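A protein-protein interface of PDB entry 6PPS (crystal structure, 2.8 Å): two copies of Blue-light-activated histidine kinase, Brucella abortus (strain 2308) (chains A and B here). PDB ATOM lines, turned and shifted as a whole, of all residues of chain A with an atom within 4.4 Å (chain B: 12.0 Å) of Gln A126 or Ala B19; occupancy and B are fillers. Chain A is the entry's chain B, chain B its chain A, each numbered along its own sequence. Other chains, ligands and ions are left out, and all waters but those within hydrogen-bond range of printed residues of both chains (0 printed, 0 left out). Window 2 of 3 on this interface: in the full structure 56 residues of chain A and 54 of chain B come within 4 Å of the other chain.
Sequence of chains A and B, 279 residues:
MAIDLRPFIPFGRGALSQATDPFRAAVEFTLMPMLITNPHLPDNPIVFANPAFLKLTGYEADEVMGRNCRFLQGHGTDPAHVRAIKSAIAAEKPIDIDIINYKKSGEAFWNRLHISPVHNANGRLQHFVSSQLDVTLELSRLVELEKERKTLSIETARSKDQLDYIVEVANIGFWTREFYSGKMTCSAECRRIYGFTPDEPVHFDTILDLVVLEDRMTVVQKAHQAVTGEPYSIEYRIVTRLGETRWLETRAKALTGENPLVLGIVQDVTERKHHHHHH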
ATOM      1  N   ASN A  38      18.949  -8.531   0.045  1.00  0.00           N
ATOM      2  CA  ASN A  38      18.781  -9.919   0.457  1.00  0.00           C
ATOM      3  C   ASN A  38      18.238 -10.000   1.879  1.00  0.00           C
ATOM      4  O   ASN A  38      18.982  -9.820   2.843  1.00  0.00           O
ATOM      5  CB  ASN A  38      20.110 -10.670   0.351  1.00  0.00           C
ATOM      6  CG  ASN A  38      19.973 -12.151   0.639  1.00  0.00           C
ATOM      7  OD1 ASN A  38      18.866 -12.691   0.678  1.00  0.00           O
ATOM      8  ND2 ASN A  38      21.102 -12.819   0.835  1.00  0.00           N
ATOM      9  N   PRO A  39      16.931 -10.269   2.013  1.00  0.00           N
ATOM     10  CA  PRO A  39      16.264 -10.326   3.318  1.00  0.00           C
ATOM     11  C   PRO A  39      16.667 -11.543   4.148  1.00  0.00           C
ATOM     12  O   PRO A  39      16.276 -11.646   5.310  1.00  0.00           O
ATOM     13  CB  PRO A  39      14.781 -10.389   2.946  1.00  0.00           C
ATOM     14  CG  PRO A  39      14.768 -11.041   1.611  1.00  0.00           C
ATOM     15  CD  PRO A  39      15.995 -10.535   0.907  1.00  0.00           C
ATOM     16  N   HIS A  40      17.432 -12.453   3.553  1.00  0.00           N
ATOM     17  CA  HIS A  40      17.903 -13.634   4.267  1.00  0.00           C
ATOM     18  C   HIS A  40      19.136 -13.304   5.098  1.00  0.00           C
ATOM     19  O   HIS A  40      19.493 -14.038   6.019  1.00  0.00           O
ATOM     20  CB  HIS A  40      18.205 -14.767   3.287  1.00  0.00           C
ATOM     21  CG  HIS A  40      16.987 -15.311   2.611  1.00  0.00           C
ATOM     22  ND1 HIS A  40      17.052 -16.234   1.588  1.00  0.00           N
ATOM     23  CD2 HIS A  40      15.670 -15.066   2.812  1.00  0.00           C
ATOM     24  CE1 HIS A  40      15.826 -16.532   1.190  1.00  0.00           C
ATOM     25  NE2 HIS A  40      14.972 -15.836   1.916  1.00  0.00           N
ATOM     26  N   VAL A 118       9.997 -10.045  -3.747  1.00  0.00           N
ATOM     27  CA  VAL A 118      10.230 -11.121  -4.705  1.00  0.00           C
ATOM     28  C   VAL A 118      10.104 -12.492  -4.045  1.00  0.00           C
ATOM     29  O   VAL A 118      10.933 -12.873  -3.220  1.00  0.00           O
ATOM     30  CB  VAL A 118      11.621 -11.003  -5.357  1.00  0.00           C
ATOM     31  CG1 VAL A 118      11.846 -12.142  -6.338  1.00  0.00           C
ATOM     32  CG2 VAL A 118      11.764  -9.661  -6.052  1.00  0.00           C
ATOM     33  N   ASN A 120       9.483 -16.822  -4.575  1.00  0.00           N
ATOM     34  CA  ASN A 120       9.714 -17.906  -5.524  1.00  0.00           C
ATOM     35  C   ASN A 120       8.453 -18.731  -5.765  1.00  0.00           C
ATOM     36  O   ASN A 120       7.340 -18.267  -5.515  1.00  0.00           O
ATOM     37  CB  ASN A 120      10.852 -18.815  -5.047  1.00  0.00           C
ATOM     38  CG  ASN A 120      10.579 -19.444  -3.692  1.00  0.00           C
ATOM     39  OD1 ASN A 120       9.505 -19.278  -3.115  1.00  0.00           O
ATOM     40  ND2 ASN A 120      11.558 -20.182  -3.180  1.00  0.00           N
ATOM     41  N   ARG A 124       8.445 -18.672  -0.883  1.00  0.00           N
ATOM     42  CA  ARG A 124       9.524 -18.269   0.008  1.00  0.00           C
ATOM     43  C   ARG A 124      10.124 -16.934  -0.427  1.00  0.00           C
ATOM     44  O   ARG A 124      10.517 -16.768  -1.583  1.00  0.00           O
ATOM     45  CB  ARG A 124      10.604 -19.354   0.049  1.00  0.00           C
ATOM     46  CG  ARG A 124      11.568 -19.247   1.218  1.00  0.00           C
ATOM     47  CD  ARG A 124      12.527 -20.433   1.255  1.00  0.00           C
ATOM     48  NE  ARG A 124      11.823 -21.714   1.253  1.00  0.00           N
ATOM     49  CZ  ARG A 124      11.812 -22.562   0.230  1.00  0.00           C
ATOM     50  NH1 ARG A 124      12.476 -22.274  -0.882  1.00  0.00           N
ATOM     51  NH2 ARG A 124      11.142 -23.703   0.319  1.00  0.00           N
ATOM     52  N   LEU A 125      10.184 -15.984   0.501  1.00  0.00           N
ATOM     53  CA  LEU A 125      10.750 -14.669   0.219  1.00  0.00           C
ATOM     54  C   LEU A 125      12.233 -14.773  -0.122  1.00  0.00           C
ATOM     55  O   LEU A 125      13.017 -15.317   0.654  1.00  0.00           O
ATOM     56  CB  LEU A 125      10.548 -13.730   1.410  1.00  0.00           C
ATOM     57  CG  LEU A 125      11.168 -12.336   1.281  1.00  0.00           C
ATOM     58  CD1 LEU A 125      10.507 -11.557   0.154  1.00  0.00           C
ATOM     59  CD2 LEU A 125      11.075 -11.574   2.594  1.00  0.00           C
ATOM     60  N   GLN A 126      12.612 -14.249  -1.283  1.00  0.00           N
ATOM     61  CA  GLN A 126      13.994 -14.345  -1.742  1.00  0.00           C
ATOM     62  C   GLN A 126      14.693 -12.990  -1.829  1.00  0.00           C
ATOM     63  O   GLN A 126      15.833 -12.849  -1.385  1.00  0.00           O
ATOM     64  CB  GLN A 126      14.057 -15.043  -3.102  1.00  0.00           C
ATOM     65  CG  GLN A 126      13.806 -16.541  -3.043  1.00  0.00           C
ATOM     66  CD  GLN A 126      14.388 -17.277  -4.235  1.00  0.00           C
ATOM     67  OE1 GLN A 126      14.968 -16.667  -5.134  1.00  0.00           O
ATOM     68  NE2 GLN A 126      14.240 -18.597  -4.246  1.00  0.00           N
ATOM     69  N   HIS A 127      14.019 -11.998  -2.400  1.00  0.00           N
ATOM     70  CA  HIS A 127      14.639 -10.691  -2.606  1.00  0.00           C
ATOM     71  C   HIS A 127      13.672  -9.521  -2.475  1.00  0.00           C
ATOM     72  O   HIS A 127      12.454  -9.696  -2.436  1.00  0.00           O
ATOM     73  CB  HIS A 127      15.297 -10.628  -3.988  1.00  0.00           C
ATOM     74  CG  HIS A 127      16.514 -11.490  -4.125  1.00  0.00           C
ATOM     75  ND1 HIS A 127      16.505 -12.685  -4.814  1.00  0.00           N
ATOM     76  CD2 HIS A 127      17.777 -11.328  -3.667  1.00  0.00           C
ATOM     77  CE1 HIS A 127      17.711 -13.221  -4.773  1.00  0.00           C
ATOM     78  NE2 HIS A 127      18.502 -12.419  -4.083  1.00  0.00           N
ATOM     79  N   ALA B  19      14.261 -20.465  -6.668  1.00  0.00           N
ATOM     80  CA  ALA B  19      15.413 -19.759  -7.217  1.00  0.00           C
ATOM     81  C   ALA B  19      14.987 -18.786  -8.310  1.00  0.00           C
ATOM     82  O   ALA B  19      14.968 -19.131  -9.492  1.00  0.00           O
ATOM     83  CB  ALA B  19      16.435 -20.750  -7.756  1.00  0.00           C
ATOM     84  N   THR B  20      14.643 -17.567  -7.907  1.00  0.00           N
ATOM     85  CA  THR B  20      14.201 -16.545  -8.849  1.00  0.00           C
ATOM     86  C   THR B  20      15.311 -15.550  -9.162  1.00  0.00           C
ATOM     87  O   THR B  20      16.063 -15.143  -8.276  1.00  0.00           O
ATOM     88  CB  THR B  20      12.980 -15.773  -8.317  1.00  0.00           C
ATOM     89  OG1 THR B  20      13.230 -15.348  -6.971  1.00  0.00           O
ATOM     90  CG2 THR B  20      11.741 -16.653  -8.343  1.00  0.00           C
ATOM     91  N   ASP B  21      15.404 -15.162 -10.429  1.00  0.00           N
ATOM     92  CA  ASP B  21      16.378 -14.171 -10.865  1.00  0.00           C
ATOM     93  C   ASP B  21      15.935 -12.775 -10.438  1.00  0.00           C
ATOM     94  O   ASP B  21      14.910 -12.277 -10.904  1.00  0.00           O
ATOM     95  CB  ASP B  21      16.562 -14.238 -12.384  1.00  0.00           C
ATOM     96  CG  ASP B  21      17.596 -13.252 -12.892  1.00  0.00           C
ATOM     97  OD1 ASP B  21      18.578 -12.989 -12.168  1.00  0.00           O
ATOM     98  OD2 ASP B  21      17.427 -12.744 -14.021  1.00  0.00           O
ATOM     99  N   PRO B  22      16.709 -12.140  -9.544  1.00  0.00           N
ATOM    100  CA  PRO B  22      16.369 -10.821  -8.996  1.00  0.00           C
ATOM    101  C   PRO B  22      16.377  -9.710 -10.047  1.00  0.00           C
ATOM    102  O   PRO B  22      15.695  -8.702  -9.863  1.00  0.00           O
ATOM    103  CB  PRO B  22      17.461 -10.586  -7.948  1.00  0.00           C
ATOM    104  CG  PRO B  22      18.600 -11.435  -8.393  1.00  0.00           C
ATOM    105  CD  PRO B  22      17.975 -12.653  -8.996  1.00  0.00           C
ATOM    106  N   PHE B  23      17.133  -9.891 -11.125  1.00  0.00           N
ATOM    107  CA  PHE B  23      17.186  -8.897 -12.193  1.00  0.00           C
ATOM    108  C   PHE B  23      15.988  -9.041 -13.127  1.00  0.00           C
ATOM    109  O   PHE B  23      15.458  -8.050 -13.629  1.00  0.00           O
ATOM    110  CB  PHE B  23      18.494  -9.014 -12.978  1.00  0.00           C
ATOM    111  CG  PHE B  23      19.720  -8.730 -12.155  1.00  0.00           C
ATOM    112  CD1 PHE B  23      20.158  -7.431 -11.968  1.00  0.00           C
ATOM    113  CD2 PHE B  23      20.428  -9.761 -11.564  1.00  0.00           C
ATOM    114  CE1 PHE B  23      21.281  -7.165 -11.207  1.00  0.00           C
ATOM    115  CE2 PHE B  23      21.553  -9.502 -10.803  1.00  0.00           C
ATOM    116  CZ  PHE B  23      21.980  -8.201 -10.625  1.00  0.00           C
ATOM    117  N   ARG B  24      15.569 -10.281 -13.355  1.00  0.00           N
ATOM    118  CA  ARG B  24      14.343 -10.556 -14.094  1.00  0.00           C
ATOM    119  C   ARG B  24      13.144  -9.989 -13.340  1.00  0.00           C
ATOM    120  O   ARG B  24      12.237  -9.414 -13.938  1.00  0.00           O
ATOM    121  CB  ARG B  24      14.176 -12.061 -14.315  1.00  0.00           C
ATOM    122  CG  ARG B  24      12.804 -12.482 -14.824  1.00  0.00           C
ATOM    123  CD  ARG B  24      12.581 -12.048 -16.260  1.00  0.00           C
ATOM    124  NE  ARG B  24      11.319 -12.550 -16.797  1.00  0.00           N
ATOM    125  CZ  ARG B  24      10.182 -11.862 -16.805  1.00  0.00           C
ATOM    126  NH1 ARG B  24      10.145 -10.635 -16.306  1.00  0.00           N
ATOM    127  NH2 ARG B  24       9.083 -12.400 -17.316  1.00  0.00           N
ATOM    128  N   ALA B  25      13.158 -10.151 -12.020  1.00  0.00           N
ATOM    129  CA  ALA B  25      12.079  -9.662 -11.169  1.00  0.00           C
ATOM    130  C   ALA B  25      12.122  -8.145 -11.034  1.00  0.00           C
ATOM    131  O   ALA B  25      11.096  -7.505 -10.805  1.00  0.00           O
ATOM    132  CB  ALA B  25      12.151 -10.315  -9.799  1.00  0.00           C
ATOM    133  N   ALA B  26      13.315  -7.574 -11.172  1.00  0.00           N
ATOM    134  CA  ALA B  26      13.480  -6.125 -11.106  1.00  0.00           C
ATOM    135  C   ALA B  26      12.841  -5.460 -12.320  1.00  0.00           C
ATOM    136  O   ALA B  26      12.110  -4.477 -12.190  1.00  0.00           O
ATOM    137  CB  ALA B  26      14.952  -5.760 -11.012  1.00  0.00           C
ATOM    138  N   PHE B  29       8.935  -5.887 -12.074  1.00  0.00           N
ATOM    139  CA  PHE B  29       8.160  -5.146 -11.085  1.00  0.00           C
ATOM    140  C   PHE B  29       8.386  -3.632 -11.104  1.00  0.00           C
ATOM    141  O   PHE B  29       7.748  -2.904 -10.343  1.00  0.00           O
ATOM    142  CB  PHE B  29       8.466  -5.684  -9.683  1.00  0.00           C
ATOM    143  CG  PHE B  29       8.020  -7.102  -9.468  1.00  0.00           C
ATOM    144  CD1 PHE B  29       6.875  -7.581 -10.080  1.00  0.00           C
ATOM    145  CD2 PHE B  29       8.749  -7.957  -8.657  1.00  0.00           C
ATOM    146  CE1 PHE B  29       6.462  -8.886  -9.886  1.00  0.00           C
ATOM    147  CE2 PHE B  29       8.340  -9.264  -8.459  1.00  0.00           C
ATOM    148  CZ  PHE B  29       7.196  -9.727  -9.075  1.00  0.00           C
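No residue of chain B comes within 4 Å of Asn A38.
No residue of chain B comes within 4 Å of Pro A39.
Val A118 touches just these residues of chain B: Thr B20 (3.5 Å) and Ala B25 (3.8 Å).
Leu A125 touches none of the printed residues of chain B.
Gln A126 touches just these residues of chain B: Ala B19 (3.1 Å) and Thr B20 (2.9 Å).
His A127 touches just one residue of chain B: Pro B22.
Of chain A, only Gln A126 (3.1 Å) comes within 4 Å of Ala B19.
Of the printed residues of chain A, Thr B20 touches Val A118, Asn A120 and Gln A126.
Printed residues of chain A within 4 Å of Pro B22: His A127 (3.9 Å).
Phe B23 touches none of the printed residues of chain A.
Of the printed residues of chain A, Ala B25 touches Val A118.
The nearest printed residue of chain A that does not touch Ala B25 is His A127 (6.6 Å).
The side-chain amide oxygen (OD1) of Asn A120 lies within hydrogen-bond range of the backbone NH (N) of Arg A124 (2.5 Å).
N of Val A118 sits at hydrogen-bond distance from O of His A127 (2.8 Å).
NE2 of Gln A126 sits close to ND2 of Asn A120, at 3.3 Å.
The backbone carbonyl oxygen (O) of Val A118 lies within hydrogen-bond range of the backbone NH (N) of Gln A126 (2.9 Å).
CG1 of Val A118 touches OG1 of Thr B20, 3.5 Å away.
Ala B25 touches Val A118.
Thr B20 touches Asn A120.
CB of Pro B22 touches ND1 of His A127, 3.9 Å away.
No position is printed for both chains.
Of the 6 pairs that touch across the chains among the printed residues, none has its exchanged pair printed and touching as well.
Hydrophobic or aromatic side chains of chain B that line the printed part of chain A: Pro B22 and Ala B25.
Along chain B the printed residues that touch a printed residue of chain A span positions 19 to 25.
Of the 9 printed residues of chain A, 4 touch a printed residue of chain B.
Printed residues of chain A that touch a printed residue of chain B: Val A118, Asn A120, Gln A126 and His A127.
Hydrophobic or aromatic side chains of chain A that line the printed part of chain B: Val A118 and His A127.
Among the printed residues, no Asp or Glu carboxylate lies within 4 Å of a Lys or Arg side-chain nitrogen of the other chain.
N of Ala B19 lies close to NE2 of Gln A126 (3.1 Å).
OG1 of Thr B20 is in hydrogen-bond range of OE1 of Gln A126.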
